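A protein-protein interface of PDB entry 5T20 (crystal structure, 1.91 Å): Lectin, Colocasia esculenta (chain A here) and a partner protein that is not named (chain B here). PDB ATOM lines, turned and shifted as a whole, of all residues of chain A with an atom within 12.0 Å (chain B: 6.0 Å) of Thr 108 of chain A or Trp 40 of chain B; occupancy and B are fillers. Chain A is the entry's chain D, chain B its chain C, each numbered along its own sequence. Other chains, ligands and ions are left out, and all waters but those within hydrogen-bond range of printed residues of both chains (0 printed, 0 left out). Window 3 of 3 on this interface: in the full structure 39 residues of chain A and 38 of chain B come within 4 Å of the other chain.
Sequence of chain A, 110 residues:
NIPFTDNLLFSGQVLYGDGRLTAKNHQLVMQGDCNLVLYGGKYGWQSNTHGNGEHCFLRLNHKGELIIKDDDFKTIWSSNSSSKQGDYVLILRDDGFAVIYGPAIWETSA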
ATOM      1  N   PHE A  10      31.828 -25.601 -20.222  1.00  0.00           N
ATOM      2  CA  PHE A  10      30.858 -25.824 -21.288  1.00  0.00           C
ATOM      3  C   PHE A  10      31.419 -25.393 -22.608  1.00  0.00           C
ATOM      4  O   PHE A  10      32.317 -24.544 -22.639  1.00  0.00           O
ATOM      5  CB  PHE A  10      29.555 -25.022 -21.006  1.00  0.00           C
ATOM      6  CG  PHE A  10      28.752 -25.553 -19.850  1.00  0.00           C
ATOM      7  CD1 PHE A  10      27.858 -26.608 -20.024  1.00  0.00           C
ATOM      8  CD2 PHE A  10      28.909 -25.027 -18.573  1.00  0.00           C
ATOM      9  CE1 PHE A  10      27.144 -27.129 -18.938  1.00  0.00           C
ATOM     10  CE2 PHE A  10      28.197 -25.551 -17.488  1.00  0.00           C
ATOM     11  CZ  PHE A  10      27.318 -26.590 -17.676  1.00  0.00           C
ATOM     12  N   ASP A  87      25.841 -29.192 -27.972  1.00  0.00           N
ATOM     13  CA  ASP A  87      26.450 -28.626 -26.765  1.00  0.00           C
ATOM     14  C   ASP A  87      27.144 -29.714 -25.933  1.00  0.00           C
ATOM     15  O   ASP A  87      26.562 -30.744 -25.631  1.00  0.00           O
ATOM     16  CB  ASP A  87      25.399 -27.894 -25.905  1.00  0.00           C
ATOM     17  CG  ASP A  87      24.723 -26.728 -26.624  1.00  0.00           C
ATOM     18  OD1 ASP A  87      25.419 -26.001 -27.347  1.00  0.00           O
ATOM     19  OD2 ASP A  87      23.497 -26.569 -26.475  1.00  0.00           O
ATOM     20  N   ALA A 104      24.296 -32.464 -25.867  1.00  0.00           N
ATOM     21  CA  ALA A 104      23.154 -32.346 -24.970  1.00  0.00           C
ATOM     22  C   ALA A 104      21.953 -33.023 -25.659  1.00  0.00           C
ATOM     23  O   ALA A 104      21.696 -32.733 -26.838  1.00  0.00           O
ATOM     24  CB  ALA A 104      22.860 -30.874 -24.700  1.00  0.00           C
ATOM     25  N   ILE A 105      21.265 -33.965 -24.964  1.00  0.00           N
ATOM     26  CA  ILE A 105      20.130 -34.683 -25.577  1.00  0.00           C
ATOM     27  C   ILE A 105      18.793 -34.307 -24.942  1.00  0.00           C
ATOM     28  O   ILE A 105      17.743 -34.616 -25.500  1.00  0.00           O
ATOM     29  CB  ILE A 105      20.318 -36.230 -25.560  1.00  0.00           C
ATOM     30  CG1 ILE A 105      20.362 -36.824 -24.121  1.00  0.00           C
ATOM     31  CG2 ILE A 105      21.497 -36.658 -26.420  1.00  0.00           C
ATOM     32  CD1 ILE A 105      20.069 -38.356 -24.034  1.00  0.00           C
ATOM     33  N   TRP A 106      18.820 -33.702 -23.749  1.00  0.00           N
ATOM     34  CA  TRP A 106      17.592 -33.359 -23.038  1.00  0.00           C
ATOM     35  C   TRP A 106      17.862 -32.232 -22.099  1.00  0.00           C
ATOM     36  O   TRP A 106      18.941 -32.173 -21.496  1.00  0.00           O
ATOM     37  CB  TRP A 106      17.036 -34.591 -22.277  1.00  0.00           C
ATOM     38  CG  TRP A 106      15.746 -34.370 -21.536  1.00  0.00           C
ATOM     39  CD1 TRP A 106      14.479 -34.579 -22.000  1.00  0.00           C
ATOM     40  CD2 TRP A 106      15.609 -33.880 -20.196  1.00  0.00           C
ATOM     41  NE1 TRP A 106      13.559 -34.233 -21.033  1.00  0.00           N
ATOM     42  CE2 TRP A 106      14.226 -33.792 -19.920  1.00  0.00           C
ATOM     43  CE3 TRP A 106      16.528 -33.469 -19.211  1.00  0.00           C
ATOM     44  CZ2 TRP A 106      13.739 -33.338 -18.695  1.00  0.00           C
ATOM     45  CZ3 TRP A 106      16.041 -33.009 -17.997  1.00  0.00           C
ATOM     46  CH2 TRP A 106      14.661 -32.986 -17.736  1.00  0.00           C
ATOM     47  N   GLU A 107      16.866 -31.351 -21.934  1.00  0.00           N
ATOM     48  CA  GLU A 107      16.972 -30.221 -21.008  1.00  0.00           C
ATOM     49  C   GLU A 107      15.600 -29.889 -20.423  1.00  0.00           C
ATOM     50  O   GLU A 107      14.585 -30.151 -21.067  1.00  0.00           O
ATOM     51  CB  GLU A 107      17.579 -28.992 -21.710  1.00  0.00           C
ATOM     52  CG  GLU A 107      16.800 -28.563 -22.952  1.00  0.00           C
ATOM     53  CD  GLU A 107      17.344 -27.403 -23.760  1.00  0.00           C
ATOM     54  OE1 GLU A 107      18.506 -26.996 -23.527  1.00  0.00           O
ATOM     55  OE2 GLU A 107      16.611 -26.919 -24.652  1.00  0.00           O
ATOM     56  N   THR A 108      15.579 -29.278 -19.219  1.00  0.00           N
ATOM     57  CA  THR A 108      14.344 -28.865 -18.540  1.00  0.00           C
ATOM     58  C   THR A 108      13.692 -27.664 -19.245  1.00  0.00           C
ATOM     59  O   THR A 108      12.472 -27.534 -19.188  1.00  0.00           O
ATOM     60  CB  THR A 108      14.587 -28.570 -17.049  1.00  0.00           C
ATOM     61  OG1 THR A 108      15.709 -27.708 -16.906  1.00  0.00           O
ATOM     62  CG2 THR A 108      14.854 -29.831 -16.244  1.00  0.00           C
ATOM     63  N   SER A 109      14.465 -26.801 -19.930  1.00  0.00           N
ATOM     64  CA  SER A 109      13.844 -25.662 -20.628  1.00  0.00           C
ATOM     65  C   SER A 109      14.596 -25.309 -21.901  1.00  0.00           C
ATOM     66  O   SER A 109      15.820 -25.320 -21.900  1.00  0.00           O
ATOM     67  CB  SER A 109      13.742 -24.438 -19.716  1.00  0.00           C
ATOM     68  OG  SER A 109      14.997 -23.827 -19.473  1.00  0.00           O
ATOM     69  N   LEU B  25      18.056 -28.437  -7.214  1.00  0.00           N
ATOM     70  CA  LEU B  25      17.308 -29.594  -7.687  1.00  0.00           C
ATOM     71  C   LEU B  25      17.159 -30.597  -6.565  1.00  0.00           C
ATOM     72  O   LEU B  25      18.160 -31.078  -6.029  1.00  0.00           O
ATOM     73  CB  LEU B  25      17.985 -30.228  -8.901  1.00  0.00           C
ATOM     74  CG  LEU B  25      17.257 -31.462  -9.548  1.00  0.00           C
ATOM     75  CD1 LEU B  25      16.084 -31.030 -10.423  1.00  0.00           C
ATOM     76  CD2 LEU B  25      18.240 -32.295 -10.395  1.00  0.00           C
ATOM     77  N   LEU B  33      10.365 -34.292  -8.238  1.00  0.00           N
ATOM     78  CA  LEU B  33      11.733 -33.839  -8.519  1.00  0.00           C
ATOM     79  C   LEU B  33      11.607 -32.382  -8.884  1.00  0.00           C
ATOM     80  O   LEU B  33      11.031 -32.075  -9.917  1.00  0.00           O
ATOM     81  CB  LEU B  33      12.402 -34.688  -9.627  1.00  0.00           C
ATOM     82  CG  LEU B  33      13.792 -34.233 -10.137  1.00  0.00           C
ATOM     83  CD1 LEU B  33      14.906 -34.485  -9.081  1.00  0.00           C
ATOM     84  CD2 LEU B  33      14.168 -34.998 -11.418  1.00  0.00           C
ATOM     85  N   VAL B  34      12.041 -31.479  -7.988  1.00  0.00           N
ATOM     86  CA  VAL B  34      11.797 -30.051  -8.160  1.00  0.00           C
ATOM     87  C   VAL B  34      13.090 -29.272  -8.309  1.00  0.00           C
ATOM     88  O   VAL B  34      13.981 -29.380  -7.463  1.00  0.00           O
ATOM     89  CB  VAL B  34      10.946 -29.471  -6.982  1.00  0.00           C
ATOM     90  CG1 VAL B  34      10.639 -27.988  -7.198  1.00  0.00           C
ATOM     91  CG2 VAL B  34       9.658 -30.255  -6.778  1.00  0.00           C
ATOM     92  N   LEU B  35      13.154 -28.456  -9.373  1.00  0.00           N
ATOM     93  CA  LEU B  35      14.253 -27.542  -9.664  1.00  0.00           C
ATOM     94  C   LEU B  35      13.855 -26.167  -9.103  1.00  0.00           C
ATOM     95  O   LEU B  35      13.221 -25.367  -9.786  1.00  0.00           O
ATOM     96  CB  LEU B  35      14.534 -27.522 -11.181  1.00  0.00           C
ATOM     97  CG  LEU B  35      15.707 -26.668 -11.763  1.00  0.00           C
ATOM     98  CD1 LEU B  35      16.881 -26.530 -10.803  1.00  0.00           C
ATOM     99  CD2 LEU B  35      16.176 -27.228 -13.099  1.00  0.00           C
ATOM    100  N   TYR B  36      14.169 -25.932  -7.824  1.00  0.00           N
ATOM    101  CA  TYR B  36      13.827 -24.683  -7.152  1.00  0.00           C
ATOM    102  C   TYR B  36      14.552 -23.527  -7.797  1.00  0.00           C
ATOM    103  O   TYR B  36      15.737 -23.647  -8.102  1.00  0.00           O
ATOM    104  CB  TYR B  36      14.089 -24.769  -5.640  1.00  0.00           C
ATOM    105  CG  TYR B  36      13.004 -25.586  -4.970  1.00  0.00           C
ATOM    106  CD1 TYR B  36      11.746 -25.043  -4.727  1.00  0.00           C
ATOM    107  CD2 TYR B  36      13.214 -26.922  -4.637  1.00  0.00           C
ATOM    108  CE1 TYR B  36      10.729 -25.799  -4.140  1.00  0.00           C
ATOM    109  CE2 TYR B  36      12.216 -27.677  -4.015  1.00  0.00           C
ATOM    110  CZ  TYR B  36      10.977 -27.105  -3.755  1.00  0.00           C
ATOM    111  OH  TYR B  36       9.951 -27.815  -3.162  1.00  0.00           O
ATOM    112  N   GLY B  38      14.074 -22.638 -10.796  1.00  0.00           N
ATOM    113  CA  GLY B  38      14.234 -22.986 -12.202  1.00  0.00           C
ATOM    114  C   GLY B  38      12.937 -23.242 -12.935  1.00  0.00           C
ATOM    115  O   GLY B  38      12.963 -23.692 -14.084  1.00  0.00           O
ATOM    116  N   ASN B  39      11.793 -22.967 -12.279  1.00  0.00           N
ATOM    117  CA  ASN B  39      10.430 -23.113 -12.824  1.00  0.00           C
ATOM    118  C   ASN B  39      10.259 -24.473 -13.528  1.00  0.00           C
ATOM    119  O   ASN B  39       9.825 -24.550 -14.678  1.00  0.00           O
ATOM    120  CB  ASN B  39      10.125 -21.937 -13.772  1.00  0.00           C
ATOM    121  CG  ASN B  39       8.684 -21.793 -14.184  1.00  0.00           C
ATOM    122  OD1 ASN B  39       7.751 -22.001 -13.404  1.00  0.00           O
ATOM    123  ND2 ASN B  39       8.477 -21.426 -15.433  1.00  0.00           N
ATOM    124  N   TRP B  40      10.689 -25.550 -12.854  1.00  0.00           N
ATOM    125  CA  TRP B  40      10.568 -26.875 -13.426  1.00  0.00           C
ATOM    126  C   TRP B  40      10.429 -27.894 -12.323  1.00  0.00           C
ATOM    127  O   TRP B  40      11.101 -27.803 -11.285  1.00  0.00           O
ATOM    128  CB  TRP B  40      11.775 -27.217 -14.341  1.00  0.00           C
ATOM    129  CG  TRP B  40      11.571 -28.490 -15.101  1.00  0.00           C
ATOM    130  CD1 TRP B  40      10.991 -28.624 -16.330  1.00  0.00           C
ATOM    131  CD2 TRP B  40      11.847 -29.823 -14.634  1.00  0.00           C
ATOM    132  NE1 TRP B  40      10.935 -29.952 -16.682  1.00  0.00           N
ATOM    133  CE2 TRP B  40      11.443 -30.713 -15.656  1.00  0.00           C
ATOM    134  CE3 TRP B  40      12.439 -30.351 -13.469  1.00  0.00           C
ATOM    135  CZ2 TRP B  40      11.609 -32.097 -15.549  1.00  0.00           C
ATOM    136  CZ3 TRP B  40      12.554 -31.724 -13.342  1.00  0.00           C
ATOM    137  CH2 TRP B  40      12.168 -32.584 -14.386  1.00  0.00           C
ATOM    138  N   GLN B  41       9.553 -28.879 -12.569  1.00  0.00           N
ATOM    139  CA  GLN B  41       9.324 -30.037 -11.706  1.00  0.00           C
ATOM    140  C   GLN B  41       8.882 -31.206 -12.565  1.00  0.00           C
ATOM    141  O   GLN B  41       8.343 -30.980 -13.652  1.00  0.00           O
ATOM    142  CB  GLN B  41       8.297 -29.741 -10.592  1.00  0.00           C
ATOM    143  CG  GLN B  41       6.953 -29.234 -11.090  1.00  0.00           C
ATOM    144  CD  GLN B  41       5.941 -29.181  -9.984  1.00  0.00           C
ATOM    145  OE1 GLN B  41       5.369 -30.199  -9.577  1.00  0.00           O
ATOM    146  NE2 GLN B  41       5.669 -27.980  -9.501  1.00  0.00           N
ATOM    147  N   SER B  42       9.092 -32.445 -12.085  1.00  0.00           N
ATOM    148  CA  SER B  42       8.641 -33.671 -12.781  1.00  0.00           C
ATOM    149  C   SER B  42       7.120 -33.822 -12.666  1.00  0.00           C
ATOM    150  O   SER B  42       6.524 -34.553 -13.461  1.00  0.00           O
ATOM    151  CB  SER B  42       9.340 -34.912 -12.225  1.00  0.00           C
ATOM    152  OG  SER B  42       9.127 -35.086 -10.831  1.00  0.00           O
ATOM    153  N   TRP B  72       8.547 -41.790 -13.361  1.00  0.00           N
ATOM    154  CA  TRP B  72       8.718 -40.769 -14.403  1.00  0.00           C
ATOM    155  C   TRP B  72      10.006 -41.025 -15.172  1.00  0.00           C
ATOM    156  O   TRP B  72      10.951 -41.573 -14.613  1.00  0.00           O
ATOM    157  CB  TRP B  72       8.753 -39.373 -13.735  1.00  0.00           C
ATOM    158  CG  TRP B  72       8.993 -38.196 -14.646  1.00  0.00           C
ATOM    159  CD1 TRP B  72       8.044 -37.416 -15.244  1.00  0.00           C
ATOM    160  CD2 TRP B  72      10.265 -37.638 -15.021  1.00  0.00           C
ATOM    161  NE1 TRP B  72       8.646 -36.421 -15.987  1.00  0.00           N
ATOM    162  CE2 TRP B  72      10.008 -36.537 -15.868  1.00  0.00           C
ATOM    163  CE3 TRP B  72      11.602 -38.003 -14.778  1.00  0.00           C
ATOM    164  CZ2 TRP B  72      11.042 -35.762 -16.425  1.00  0.00           C
ATOM    165  CZ3 TRP B  72      12.622 -37.220 -15.303  1.00  0.00           C
ATOM    166  CH2 TRP B  72      12.342 -36.131 -16.136  1.00  0.00           C
ATOM    167  N   GLY B  91      20.368 -22.279 -14.816  1.00  0.00           N
ATOM    168  CA  GLY B  91      19.206 -22.919 -14.214  1.00  0.00           C
ATOM    169  C   GLY B  91      18.418 -23.935 -14.995  1.00  0.00           C
ATOM    170  O   GLY B  91      17.195 -24.011 -14.859  1.00  0.00           O
ATOM    171  N   ARG B  92      19.107 -24.715 -15.796  1.00  0.00           N
ATOM    172  CA  ARG B  92      18.522 -25.828 -16.538  1.00  0.00           C
ATOM    173  C   ARG B  92      19.230 -27.090 -16.114  1.00  0.00           C
ATOM    174  O   ARG B  92      20.446 -27.053 -15.907  1.00  0.00           O
ATOM    175  CB  ARG B  92      18.718 -25.644 -18.054  1.00  0.00           C
ATOM    176  CG  ARG B  92      18.115 -24.389 -18.669  1.00  0.00           C
ATOM    177  CD  ARG B  92      18.299 -24.359 -20.183  1.00  0.00           C
ATOM    178  NE  ARG B  92      19.663 -24.658 -20.642  1.00  0.00           N
ATOM    179  CZ  ARG B  92      20.633 -23.757 -20.771  1.00  0.00           C
ATOM    180  NH1 ARG B  92      20.425 -22.491 -20.421  1.00  0.00           N
ATOM    181  NH2 ARG B  92      21.825 -24.119 -21.217  1.00  0.00           N
ATOM    182  N   LEU B  93      18.520 -28.215 -16.055  1.00  0.00           N
ATOM    183  CA  LEU B  93      19.179 -29.502 -15.828  1.00  0.00           C
ATOM    184  C   LEU B  93      19.316 -30.090 -17.228  1.00  0.00           C
ATOM    185  O   LEU B  93      18.324 -30.126 -17.968  1.00  0.00           O
ATOM    186  CB  LEU B  93      18.425 -30.424 -14.837  1.00  0.00           C
ATOM    187  CG  LEU B  93      19.006 -31.826 -14.672  1.00  0.00           C
ATOM    188  CD1 LEU B  93      20.277 -31.814 -13.805  1.00  0.00           C
ATOM    189  CD2 LEU B  93      17.944 -32.819 -14.179  1.00  0.00           C
ATOM    190  N   VAL B  94      20.550 -30.448 -17.625  1.00  0.00           N
ATOM    191  CA  VAL B  94      20.847 -30.898 -18.993  1.00  0.00           C
ATOM    192  C   VAL B  94      21.542 -32.248 -18.994  1.00  0.00           C
ATOM    193  O   VAL B  94      22.534 -32.430 -18.295  1.00  0.00           O
ATOM    194  CB  VAL B  94      21.713 -29.847 -19.754  1.00  0.00           C
ATOM    195  CG1 VAL B  94      21.916 -30.250 -21.219  1.00  0.00           C
ATOM    196  CG2 VAL B  94      21.103 -28.433 -19.663  1.00  0.00           C
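The side-chain hydroxyl of Thr 108 of chain A is in hydrogen-bond range of the backbone NH of Leu 93 of chain B, at 3.0 Å. The side-chain carboxylate (OE1) of Glu 107 of chain A lies within salt-bridge range of the guanidinium group (NE) of Arg 92 of chain B (3.9 Å).
O of Asp 87 of chain A sits at hydrogen-bond distance from N of Ala 104 of chain A (2.9 Å). O of Trp 40 of chain B lies within hydrogen-bond range of N of Leu 35 of chain B (2.9 Å).
Among the printed residues, pairs that only touch across the chains: Ser 109 of chain A with Arg 92 of chain B (3.2 Å), Glu 107 of chain A with Leu 93 of chain B (3.3 Å), Trp 106 of chain A with Val 94 of chain B (3.4 Å), Thr 108 of chain A with Trp 40 of chain B (3.4 Å), Thr 108 of chain A with Arg 92 of chain B (3.4 Å), Ala 104 of chain A with Val 94 of chain B (3.7 Å), Trp 106 of chain A with Leu 93 of chain B (3.7 Å), Trp 106 of chain A with Trp 40 of chain B (3.9 Å) and Thr 108 of chain A with Leu 35 of chain B (3.9 Å).
Printed residues of chain B within 4 Å of Thr 108 of chain A: Leu 35 (3.9 Å), Trp 40 (3.4 Å), Arg 92 (3.4 Å) and Leu 93 (3.0 Å). Of the printed residues of chain A, Trp 40 of chain B touches Trp 106 (3.9 Å) and Thr 108 (3.4 Å). Leu 33 of chain B touches none of the printed residues of chain A. No residue of chain A comes within 4 Å of Val 34 of chain B. Of chain A, only Thr 108 comes within 4 Å of Leu 35 of chain B. No residue of chain A comes within 4 Å of Gly 38 of chain B. No residue of chain A comes within 4 Å of Gln 41 of chain B. No residue of chain A comes within 4 Å of Ser 42 of chain B. Leu 93 of chain B touches just these residues of chain A: Trp 106 (3.7 Å), Glu 107 (3.3 Å) and Thr 108 (3.0 Å). Of chain A, only Ala 104 (3.7 Å) and Trp 106 (3.4 Å) come within 4 Å of Val 94 of chain B. Printed residues of chain B within 4 Å of Ala 104 of chain A: Val 94. Of the printed residues of chain B, Glu 107 of chain A touches Arg 92 and Leu 93. Of the printed residues of chain A, Arg 92 of chain B touches Glu 107, Thr 108 and Ser 109. Of the printed residues of chain B, Ser 109 of chain A touches Arg 92. Asp 87 of chain A touches none of the printed residues of chain B. The nearest printed residue of chain B that does not touch Trp 106 of chain A is Trp 72 of chain B (4.04 Å).
Of the 15 printed residues of chain B, 5 touch a printed residue of chain A. Printed residues of chain B that touch a printed residue of chain A: Leu 35, Trp 40, Arg 92, Leu 93 and Val 94. Of the 8 printed residues of chain A, 5 touch a printed residue of chain B.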
